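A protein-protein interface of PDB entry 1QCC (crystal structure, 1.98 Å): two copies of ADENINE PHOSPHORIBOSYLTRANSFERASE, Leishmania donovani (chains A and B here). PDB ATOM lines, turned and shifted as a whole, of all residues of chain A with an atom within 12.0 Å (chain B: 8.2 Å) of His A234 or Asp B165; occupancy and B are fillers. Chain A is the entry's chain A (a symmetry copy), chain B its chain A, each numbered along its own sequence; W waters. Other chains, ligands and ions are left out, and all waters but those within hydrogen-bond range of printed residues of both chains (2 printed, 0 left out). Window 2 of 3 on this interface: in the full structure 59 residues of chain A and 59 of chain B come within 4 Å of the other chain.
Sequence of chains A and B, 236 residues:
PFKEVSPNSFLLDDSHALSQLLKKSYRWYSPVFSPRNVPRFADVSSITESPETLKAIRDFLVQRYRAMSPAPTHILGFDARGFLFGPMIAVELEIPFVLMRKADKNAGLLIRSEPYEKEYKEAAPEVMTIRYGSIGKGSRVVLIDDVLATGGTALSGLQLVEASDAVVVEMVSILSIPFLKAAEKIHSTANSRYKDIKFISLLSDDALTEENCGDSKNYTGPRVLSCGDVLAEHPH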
ATOM      1  N   LEU A 225      -5.624  16.018 -10.076  1.00  0.00           N
ATOM      2  CA  LEU A 225      -5.750  15.386 -11.385  1.00  0.00           C
ATOM      3  C   LEU A 225      -5.340  16.386 -12.468  1.00  0.00           C
ATOM      4  O   LEU A 225      -5.638  17.574 -12.358  1.00  0.00           O
ATOM      5  CB  LEU A 225      -7.204  14.952 -11.623  1.00  0.00           C
ATOM      6  CG  LEU A 225      -7.891  13.974 -10.660  1.00  0.00           C
ATOM      7  CD1 LEU A 225      -8.319  14.668  -9.361  1.00  0.00           C
ATOM      8  CD2 LEU A 225      -9.112  13.397 -11.356  1.00  0.00           C
ATOM      9  N   SER A 226      -4.643  15.916 -13.501  1.00  0.00           N
ATOM     10  CA  SER A 226      -4.227  16.797 -14.595  1.00  0.00           C
ATOM     11  C   SER A 226      -5.442  17.118 -15.466  1.00  0.00           C
ATOM     12  O   SER A 226      -6.403  16.341 -15.504  1.00  0.00           O
ATOM     13  CB  SER A 226      -3.132  16.136 -15.439  1.00  0.00           C
ATOM     14  OG  SER A 226      -3.622  14.976 -16.088  1.00  0.00           O
ATOM     15  N   CYS A 227      -5.419  18.257 -16.151  1.00  0.00           N
ATOM     16  CA  CYS A 227      -6.550  18.618 -16.999  1.00  0.00           C
ATOM     17  C   CYS A 227      -6.747  17.619 -18.147  1.00  0.00           C
ATOM     18  O   CYS A 227      -7.873  17.375 -18.576  1.00  0.00           O
ATOM     19  CB  CYS A 227      -6.470  20.085 -17.474  1.00  0.00           C
ATOM     20  SG  CYS A 227      -4.954  20.601 -18.256  1.00  0.00           S
ATOM     21  N   GLY A 228      -5.660  16.982 -18.580  1.00  0.00           N
ATOM     22  CA  GLY A 228      -5.745  15.984 -19.636  1.00  0.00           C
ATOM     23  C   GLY A 228      -6.506  14.760 -19.143  1.00  0.00           C
ATOM     24  O   GLY A 228      -7.326  14.194 -19.861  1.00  0.00           O
ATOM     25  N   ASP A 229      -6.249  14.351 -17.904  1.00  0.00           N
ATOM     26  CA  ASP A 229      -6.934  13.202 -17.318  1.00  0.00           C
ATOM     27  C   ASP A 229      -8.430  13.473 -17.134  1.00  0.00           C
ATOM     28  O   ASP A 229      -9.257  12.596 -17.378  1.00  0.00           O
ATOM     29  CB  ASP A 229      -6.307  12.819 -15.968  1.00  0.00           C
ATOM     30  CG  ASP A 229      -4.960  12.102 -16.116  1.00  0.00           C
ATOM     31  OD1 ASP A 229      -4.290  11.883 -15.082  1.00  0.00           O
ATOM     32  OD2 ASP A 229      -4.571  11.753 -17.253  1.00  0.00           O
ATOM     33  N   VAL A 230      -8.773  14.683 -16.699  1.00  0.00           N
ATOM     34  CA  VAL A 230     -10.172  15.056 -16.491  1.00  0.00           C
ATOM     35  C   VAL A 230     -10.896  15.121 -17.836  1.00  0.00           C
ATOM     36  O   VAL A 230     -12.072  14.760 -17.932  1.00  0.00           O
ATOM     37  CB  VAL A 230     -10.290  16.401 -15.720  1.00  0.00           C
ATOM     38  CG1 VAL A 230     -11.752  16.756 -15.468  1.00  0.00           C
ATOM     39  CG2 VAL A 230      -9.558  16.296 -14.392  1.00  0.00           C
ATOM     40  N   LEU A 231     -10.177  15.536 -18.878  1.00  0.00           N
ATOM     41  CA  LEU A 231     -10.737  15.614 -20.228  1.00  0.00           C
ATOM     42  C   LEU A 231     -11.195  14.244 -20.741  1.00  0.00           C
ATOM     43  O   LEU A 231     -12.250  14.129 -21.360  1.00  0.00           O
ATOM     44  CB  LEU A 231      -9.715  16.209 -21.203  1.00  0.00           C
ATOM     45  CG  LEU A 231      -9.779  17.714 -21.476  1.00  0.00           C
ATOM     46  CD1 LEU A 231      -8.603  18.130 -22.343  1.00  0.00           C
ATOM     47  CD2 LEU A 231     -11.088  18.062 -22.169  1.00  0.00           C
ATOM     48  N   ALA A 232     -10.415  13.209 -20.454  1.00  0.00           N
ATOM     49  CA  ALA A 232     -10.722  11.847 -20.885  1.00  0.00           C
ATOM     50  C   ALA A 232     -11.945  11.219 -20.201  1.00  0.00           C
ATOM     51  O   ALA A 232     -12.383  10.130 -20.582  1.00  0.00           O
ATOM     52  CB  ALA A 232      -9.502  10.963 -20.684  1.00  0.00           C
ATOM     53  N   GLU A 233     -12.491  11.900 -19.196  1.00  0.00           N
ATOM     54  CA  GLU A 233     -13.658  11.399 -18.462  1.00  0.00           C
ATOM     55  C   GLU A 233     -14.987  11.737 -19.128  1.00  0.00           C
ATOM     56  O   GLU A 233     -16.038  11.260 -18.695  1.00  0.00           O
ATOM     57  CB  GLU A 233     -13.692  11.969 -17.045  1.00  0.00           C
ATOM     58  CG  GLU A 233     -12.506  11.634 -16.161  1.00  0.00           C
ATOM     59  CD  GLU A 233     -12.613  12.278 -14.785  1.00  0.00           C
ATOM     60  OE1 GLU A 233     -11.681  12.092 -13.970  1.00  0.00           O
ATOM     61  OE2 GLU A 233     -13.622  12.971 -14.515  1.00  0.00           O
ATOM     62  N   HIS A 234     -14.949  12.590 -20.150  1.00  0.00           N
ATOM     63  CA  HIS A 234     -16.164  12.991 -20.848  1.00  0.00           C
ATOM     64  C   HIS A 234     -15.942  13.166 -22.353  1.00  0.00           C
ATOM     65  O   HIS A 234     -14.815  13.384 -22.797  1.00  0.00           O
ATOM     66  CB  HIS A 234     -16.723  14.289 -20.239  1.00  0.00           C
ATOM     67  CG  HIS A 234     -15.799  15.466 -20.347  1.00  0.00           C
ATOM     68  ND1 HIS A 234     -14.956  15.850 -19.325  1.00  0.00           N
ATOM     69  CD2 HIS A 234     -15.590  16.348 -21.356  1.00  0.00           C
ATOM     70  CE1 HIS A 234     -14.271  16.917 -19.698  1.00  0.00           C
ATOM     71  NE2 HIS A 234     -14.637  17.238 -20.925  1.00  0.00           N
ATOM     72  N   PRO A 235     -17.016  13.020 -23.158  1.00  0.00           N
ATOM     73  CA  PRO A 235     -16.923  13.171 -24.616  1.00  0.00           C
ATOM     74  C   PRO A 235     -16.547  14.609 -24.980  1.00  0.00           C
ATOM     75  O   PRO A 235     -17.200  15.563 -24.553  1.00  0.00           O
ATOM     76  CB  PRO A 235     -18.339  12.826 -25.083  1.00  0.00           C
ATOM     77  CG  PRO A 235     -18.809  11.859 -24.044  1.00  0.00           C
ATOM     78  CD  PRO A 235     -18.352  12.525 -22.775  1.00  0.00           C
ATOM     79  N   HIS A 236     -15.480  14.759 -25.753  1.00  0.00           N
ATOM     80  CA  HIS A 236     -15.017  16.080 -26.162  1.00  0.00           C
ATOM     81  C   HIS A 236     -14.379  16.050 -27.545  1.00  0.00           C
ATOM     82  O   HIS A 236     -14.368  17.120 -28.191  1.00  0.00           O
ATOM     83  CB  HIS A 236     -14.025  16.644 -25.131  1.00  0.00           C
ATOM     84  CG  HIS A 236     -12.731  15.891 -25.053  1.00  0.00           C
ATOM     85  ND1 HIS A 236     -12.602  14.697 -24.376  1.00  0.00           N
ATOM     86  CD2 HIS A 236     -11.508  16.164 -25.569  1.00  0.00           C
ATOM     87  CE1 HIS A 236     -11.356  14.267 -24.479  1.00  0.00           C
ATOM     88  NE2 HIS A 236     -10.672  15.139 -25.197  1.00  0.00           N
ATOM     89  OXT HIS A 236     -13.895  14.968 -27.960  1.00  0.00           O
ATOM     90  N   ILE B 111      -7.959  20.063 -10.074  1.00  0.00           N
ATOM     91  CA  ILE B 111      -7.633  19.816 -11.476  1.00  0.00           C
ATOM     92  C   ILE B 111      -6.452  20.750 -11.735  1.00  0.00           C
ATOM     93  O   ILE B 111      -6.562  21.945 -11.479  1.00  0.00           O
ATOM     94  CB  ILE B 111      -8.781  20.236 -12.431  1.00  0.00           C
ATOM     95  CG1 ILE B 111     -10.093  19.560 -12.029  1.00  0.00           C
ATOM     96  CG2 ILE B 111      -8.419  19.881 -13.887  1.00  0.00           C
ATOM     97  CD1 ILE B 111     -11.287  20.024 -12.840  1.00  0.00           C
ATOM     98  N   TYR B 132     -12.045  20.482  -8.341  1.00  0.00           N
ATOM     99  CA  TYR B 132     -12.793  19.631  -9.247  1.00  0.00           C
ATOM    100  C   TYR B 132     -14.281  19.853  -8.981  1.00  0.00           C
ATOM    101  O   TYR B 132     -14.741  19.709  -7.852  1.00  0.00           O
ATOM    102  CB  TYR B 132     -12.411  18.173  -8.987  1.00  0.00           C
ATOM    103  CG  TYR B 132     -13.053  17.178  -9.917  1.00  0.00           C
ATOM    104  CD1 TYR B 132     -14.345  16.705  -9.679  1.00  0.00           C
ATOM    105  CD2 TYR B 132     -12.366  16.696 -11.031  1.00  0.00           C
ATOM    106  CE1 TYR B 132     -14.940  15.776 -10.534  1.00  0.00           C
ATOM    107  CE2 TYR B 132     -12.947  15.765 -11.893  1.00  0.00           C
ATOM    108  CZ  TYR B 132     -14.233  15.310 -11.638  1.00  0.00           C
ATOM    109  OH  TYR B 132     -14.808  14.387 -12.481  1.00  0.00           O
ATOM    110  N   ILE B 135     -16.657  24.299 -11.372  1.00  0.00           N
ATOM    111  CA  ILE B 135     -17.265  24.758 -12.617  1.00  0.00           C
ATOM    112  C   ILE B 135     -17.737  23.497 -13.327  1.00  0.00           C
ATOM    113  O   ILE B 135     -16.990  22.533 -13.453  1.00  0.00           O
ATOM    114  CB  ILE B 135     -16.232  25.496 -13.499  1.00  0.00           C
ATOM    115  CG1 ILE B 135     -15.824  26.812 -12.836  1.00  0.00           C
ATOM    116  CG2 ILE B 135     -16.801  25.758 -14.883  1.00  0.00           C
ATOM    117  CD1 ILE B 135     -14.327  27.027 -12.806  1.00  0.00           C
ATOM    118  N   GLY B 136     -18.988  23.486 -13.763  1.00  0.00           N
ATOM    119  CA  GLY B 136     -19.500  22.305 -14.431  1.00  0.00           C
ATOM    120  C   GLY B 136     -19.763  22.447 -15.916  1.00  0.00           C
ATOM    121  O   GLY B 136     -19.456  23.469 -16.532  1.00  0.00           O
ATOM    122  N   LYS B 137     -20.297  21.373 -16.492  1.00  0.00           N
ATOM    123  CA  LYS B 137     -20.654  21.323 -17.904  1.00  0.00           C
ATOM    124  C   LYS B 137     -21.735  22.380 -18.113  1.00  0.00           C
ATOM    125  O   LYS B 137     -22.665  22.491 -17.311  1.00  0.00           O
ATOM    126  CB  LYS B 137     -21.197  19.928 -18.239  1.00  0.00           C
ATOM    127  CG  LYS B 137     -21.704  19.728 -19.660  1.00  0.00           C
ATOM    128  CD  LYS B 137     -22.171  18.287 -19.842  1.00  0.00           C
ATOM    129  CE  LYS B 137     -22.651  18.014 -21.258  1.00  0.00           C
ATOM    130  NZ  LYS B 137     -23.145  16.607 -21.407  1.00  0.00           N
ATOM    131  N   GLY B 138     -21.561  23.207 -19.137  1.00  0.00           N
ATOM    132  CA  GLY B 138     -22.535  24.248 -19.412  1.00  0.00           C
ATOM    133  C   GLY B 138     -22.250  25.579 -18.742  1.00  0.00           C
ATOM    134  O   GLY B 138     -22.967  26.554 -18.978  1.00  0.00           O
ATOM    135  N   SER B 139     -21.228  25.622 -17.887  1.00  0.00           N
ATOM    136  CA  SER B 139     -20.856  26.860 -17.203  1.00  0.00           C
ATOM    137  C   SER B 139     -20.201  27.807 -18.200  1.00  0.00           C
ATOM    138  O   SER B 139     -19.458  27.378 -19.077  1.00  0.00           O
ATOM    139  CB  SER B 139     -19.876  26.594 -16.053  1.00  0.00           C
ATOM    140  OG  SER B 139     -20.414  25.715 -15.080  1.00  0.00           O
ATOM    141  N   ARG B 140     -20.529  29.087 -18.081  1.00  0.00           N
ATOM    142  CA  ARG B 140     -19.980  30.127 -18.936  1.00  0.00           C
ATOM    143  C   ARG B 140     -19.163  30.989 -17.984  1.00  0.00           C
ATOM    144  O   ARG B 140     -19.702  31.749 -17.180  1.00  0.00           O
ATOM    145  CB  ARG B 140     -21.114  30.899 -19.611  1.00  0.00           C
ATOM    146  CG  ARG B 140     -21.946  30.014 -20.553  1.00  0.00           C
ATOM    147  CD  ARG B 140     -23.084  30.775 -21.222  1.00  0.00           C
ATOM    148  NE  ARG B 140     -24.113  31.217 -20.275  1.00  0.00           N
ATOM    149  CZ  ARG B 140     -25.090  30.445 -19.799  1.00  0.00           C
ATOM    150  NH1 ARG B 140     -25.186  29.171 -20.168  1.00  0.00           N
ATOM    151  NH2 ARG B 140     -26.001  30.960 -18.982  1.00  0.00           N
ATOM    152  N   VAL B 141     -17.849  30.831 -18.073  1.00  0.00           N
ATOM    153  CA  VAL B 141     -16.920  31.495 -17.177  1.00  0.00           C
ATOM    154  C   VAL B 141     -16.172  32.718 -17.675  1.00  0.00           C
ATOM    155  O   VAL B 141     -15.612  32.721 -18.774  1.00  0.00           O
ATOM    156  CB  VAL B 141     -15.856  30.485 -16.690  1.00  0.00           C
ATOM    157  CG1 VAL B 141     -15.019  31.082 -15.566  1.00  0.00           C
ATOM    158  CG2 VAL B 141     -16.516  29.189 -16.247  1.00  0.00           C
ATOM    159  N   LEU B 158      -7.766  28.930 -19.277  1.00  0.00           N
ATOM    160  CA  LEU B 158      -8.430  28.349 -20.451  1.00  0.00           C
ATOM    161  C   LEU B 158      -8.442  26.825 -20.390  1.00  0.00           C
ATOM    162  O   LEU B 158      -9.474  26.196 -20.608  1.00  0.00           O
ATOM    163  CB  LEU B 158      -7.750  28.811 -21.747  1.00  0.00           C
ATOM    164  CG  LEU B 158      -7.647  30.323 -21.967  1.00  0.00           C
ATOM    165  CD1 LEU B 158      -6.973  30.611 -23.300  1.00  0.00           C
ATOM    166  CD2 LEU B 158      -9.020  30.958 -21.907  1.00  0.00           C
ATOM    167  N   GLN B 159      -7.292  26.241 -20.074  1.00  0.00           N
ATOM    168  CA  GLN B 159      -7.162  24.792 -19.965  1.00  0.00           C
ATOM    169  C   GLN B 159      -8.084  24.210 -18.897  1.00  0.00           C
ATOM    170  O   GLN B 159      -8.729  23.195 -19.124  1.00  0.00           O
ATOM    171  CB  GLN B 159      -5.721  24.413 -19.625  1.00  0.00           C
ATOM    172  CG  GLN B 159      -4.703  24.753 -20.696  1.00  0.00           C
ATOM    173  CD  GLN B 159      -3.288  24.418 -20.266  1.00  0.00           C
ATOM    174  OE1 GLN B 159      -2.965  24.428 -19.073  1.00  0.00           O
ATOM    175  NE2 GLN B 159      -2.435  24.122 -21.239  1.00  0.00           N
ATOM    176  N   LEU B 160      -8.116  24.847 -17.728  1.00  0.00           N
ATOM    177  CA  LEU B 160      -8.942  24.398 -16.614  1.00  0.00           C
ATOM    178  C   LEU B 160     -10.441  24.485 -16.915  1.00  0.00           C
ATOM    179  O   LEU B 160     -11.196  23.591 -16.547  1.00  0.00           O
ATOM    180  CB  LEU B 160      -8.593  25.176 -15.340  1.00  0.00           C
ATOM    181  CG  LEU B 160      -7.189  24.917 -14.780  1.00  0.00           C
ATOM    182  CD1 LEU B 160      -6.853  25.906 -13.682  1.00  0.00           C
ATOM    183  CD2 LEU B 160      -7.087  23.481 -14.271  1.00  0.00           C
ATOM    184  N   VAL B 161     -10.868  25.549 -17.592  1.00  0.00           N
ATOM    185  CA  VAL B 161     -12.278  25.702 -17.949  1.00  0.00           C
ATOM    186  C   VAL B 161     -12.655  24.655 -19.011  1.00  0.00           C
ATOM    187  O   VAL B 161     -13.711  24.024 -18.932  1.00  0.00           O
ATOM    188  CB  VAL B 161     -12.583  27.136 -18.461  1.00  0.00           C
ATOM    189  CG1 VAL B 161     -14.001  27.212 -19.009  1.00  0.00           C
ATOM    190  CG2 VAL B 161     -12.406  28.150 -17.333  1.00  0.00           C
ATOM    191  N   GLU B 162     -11.765  24.458 -19.979  1.00  0.00           N
ATOM    192  CA  GLU B 162     -11.960  23.477 -21.049  1.00  0.00           C
ATOM    193  C   GLU B 162     -12.052  22.066 -20.471  1.00  0.00           C
ATOM    194  O   GLU B 162     -12.945  21.302 -20.822  1.00  0.00           O
ATOM    195  CB  GLU B 162     -10.798  23.571 -22.045  1.00  0.00           C
ATOM    196  CG  GLU B 162     -10.714  22.460 -23.079  1.00  0.00           C
ATOM    197  CD  GLU B 162      -9.578  22.677 -24.065  1.00  0.00           C
ATOM    198  OE1 GLU B 162      -8.428  22.905 -23.622  1.00  0.00           O
ATOM    199  OE2 GLU B 162      -9.836  22.628 -25.286  1.00  0.00           O
ATOM    200  N   ALA B 163     -11.141  21.744 -19.558  1.00  0.00           N
ATOM    201  CA  ALA B 163     -11.101  20.438 -18.915  1.00  0.00           C
ATOM    202  C   ALA B 163     -12.388  20.164 -18.141  1.00  0.00           C
ATOM    203  O   ALA B 163     -12.813  19.012 -18.018  1.00  0.00           O
ATOM    204  CB  ALA B 163      -9.900  20.358 -17.981  1.00  0.00           C
ATOM    205  N   SER B 164     -12.994  21.230 -17.622  1.00  0.00           N
ATOM    206  CA  SER B 164     -14.235  21.142 -16.855  1.00  0.00           C
ATOM    207  C   SER B 164     -15.477  21.003 -17.733  1.00  0.00           C
ATOM    208  O   SER B 164     -16.597  20.950 -17.225  1.00  0.00           O
ATOM    209  CB  SER B 164     -14.384  22.377 -15.970  1.00  0.00           C
ATOM    210  OG  SER B 164     -13.334  22.448 -15.028  1.00  0.00           O
ATOM    211  N   ASP B 165     -15.269  20.968 -19.047  1.00  0.00           N
ATOM    212  CA  ASP B 165     -16.349  20.839 -20.019  1.00  0.00           C
ATOM    213  C   ASP B 165     -17.223  22.096 -20.018  1.00  0.00           C
ATOM    214  O   ASP B 165     -18.434  22.032 -20.214  1.00  0.00           O
ATOM    215  CB  ASP B 165     -17.185  19.582 -19.722  1.00  0.00           C
ATOM    216  CG  ASP B 165     -17.909  19.040 -20.954  1.00  0.00           C
ATOM    217  OD1 ASP B 165     -17.710  19.563 -22.076  1.00  0.00           O
ATOM    218  OD2 ASP B 165     -18.675  18.069 -20.794  1.00  0.00           O
ATOM    219  N   ALA B 166     -16.586  23.238 -19.794  1.00  0.00           N
ATOM    220  CA  ALA B 166     -17.266  24.530 -19.767  1.00  0.00           C
ATOM    221  C   ALA B 166     -16.638  25.440 -20.824  1.00  0.00           C
ATOM    222  O   ALA B 166     -15.629  25.082 -21.431  1.00  0.00           O
ATOM    223  CB  ALA B 166     -17.129  25.155 -18.389  1.00  0.00           C
ATOM    224  N   VAL B 167     -17.235  26.608 -21.050  1.00  0.00           N
ATOM    225  CA  VAL B 167     -16.694  27.553 -22.034  1.00  0.00           C
ATOM    226  C   VAL B 167     -16.271  28.877 -21.410  1.00  0.00           C
ATOM    227  O   VAL B 167     -16.835  29.318 -20.406  1.00  0.00           O
ATOM    228  CB  VAL B 167     -17.687  27.854 -23.203  1.00  0.00           C
ATOM    229  CG1 VAL B 167     -18.033  26.571 -23.955  1.00  0.00           C
ATOM    230  CG2 VAL B 167     -18.941  28.531 -22.686  1.00  0.00           C
ATOM    231  N   VAL B 168     -15.245  29.480 -21.999  1.00  0.00           N
ATOM    232  CA  VAL B 168     -14.730  30.761 -21.546  1.00  0.00           C
ATOM    233  C   VAL B 168     -15.507  31.867 -22.248  1.00  0.00           C
ATOM    234  O   VAL B 168     -15.616  31.870 -23.478  1.00  0.00           O
ATOM    235  CB  VAL B 168     -13.219  30.913 -21.871  1.00  0.00           C
ATOM    236  CG1 VAL B 168     -12.739  32.334 -21.568  1.00  0.00           C
ATOM    237  CG2 VAL B 168     -12.409  29.909 -21.069  1.00  0.00           C
HETATM  238  O   HOH W   1     -13.996  19.682 -22.825  1.00  0.00           O
HETATM  239  O   HOH W   2     -19.125  16.793 -23.192  1.00  0.00           O
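The side-chain carboxylate (OE2) of Glu A233 sits at hydrogen-bond distance from the side-chain hydroxyl (OH) of Tyr B132, 2.7 Å away.
A ring nitrogen (ND1) of His A236 sits at hydrogen-bond distance from the backbone carbonyl oxygen (O) of Leu A231 (3.1 Å).
The backbone carbonyl oxygen of His A234 is in hydrogen-bond range of a ring nitrogen (ND1) of His A236 (3.0 Å).
O of Val A230 sits at hydrogen-bond distance from ND1 of His A234, at 3.4 Å.
Leu A225 touches Ile B111.
Ile B111 touches Cys A227.
Cys A227 touches Ala B163 (CB to CB, 3.5 Å).
Val A230 touches Ile B111.
Tyr B132 touches Val A230.
Ala B163 touches Val A230 (O to CG1, 3.6 Å).
Leu A231 touches Glu B162 (CD2 to O, 3.97 Å).
Ala B163 touches Leu A231.
His A234 touches Ala B163.
CG of Asp B165 touches CD2 of His A234, 3.6 Å away.
Of the printed residues of chain B, Cys A227 touches Ile B111 and Ala B163.
Of the printed residues of chain B, Leu A231 touches Glu B162 (3.97 Å) and Ala B163 (3.97 Å).
Ala A232 touches none of the printed residues of chain B.
Of the printed residues of chain B, Glu A233 touches Tyr B132 (2.7 Å).
No residue of chain B comes within 4 Å of Pro A235.
Of the printed residues of chain A, Tyr B132 touches Val A230 (3.9 Å) and Glu A233 (2.7 Å).
No residue of chain A comes within 4 Å of Lys B137.
No residue of chain A comes within 4 Å of Gly B138.
No residue of chain A comes within 4 Å of Ser B139.
Ala B163 touches four residues of chain A.
No residue of chain A comes within 4 Å of Ser B164.
Asp B165 touches just one residue of chain A: His A234 (3.6 Å).
No residue of chain A comes within 4 Å of Ala B166.
No residue of chain A comes within 4 Å of Val B167.
The nearest residue of chain A that does not touch Asp B165 is Pro A235 (4.7 Å).
Of the 12 printed residues of chain A, 6 touch a printed residue of chain B.
Hydrophobic or aromatic side chains of chain A that line the printed part of chain B: Val A230, Leu A231 and His A234.
Of the 20 printed residues of chain B, 5 touch a printed residue of chain A.
Hydrophobic or aromatic side chains of chain B that line the printed part of chain A: Ile B111, Tyr B132 and Ala B163.
No position is printed for both chains.
Of the 11 pairs that touch across the chains among the printed residues, none has its exchanged pair printed and touching as well.
Water W2 bridges O of Pro A235 (2.7 Å) and OD2 of Asp B165 (2.8 Å).
Water W1 bridges O of Glu B162 (2.8 Å) and NE2 of His A234 (3.2 Å).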
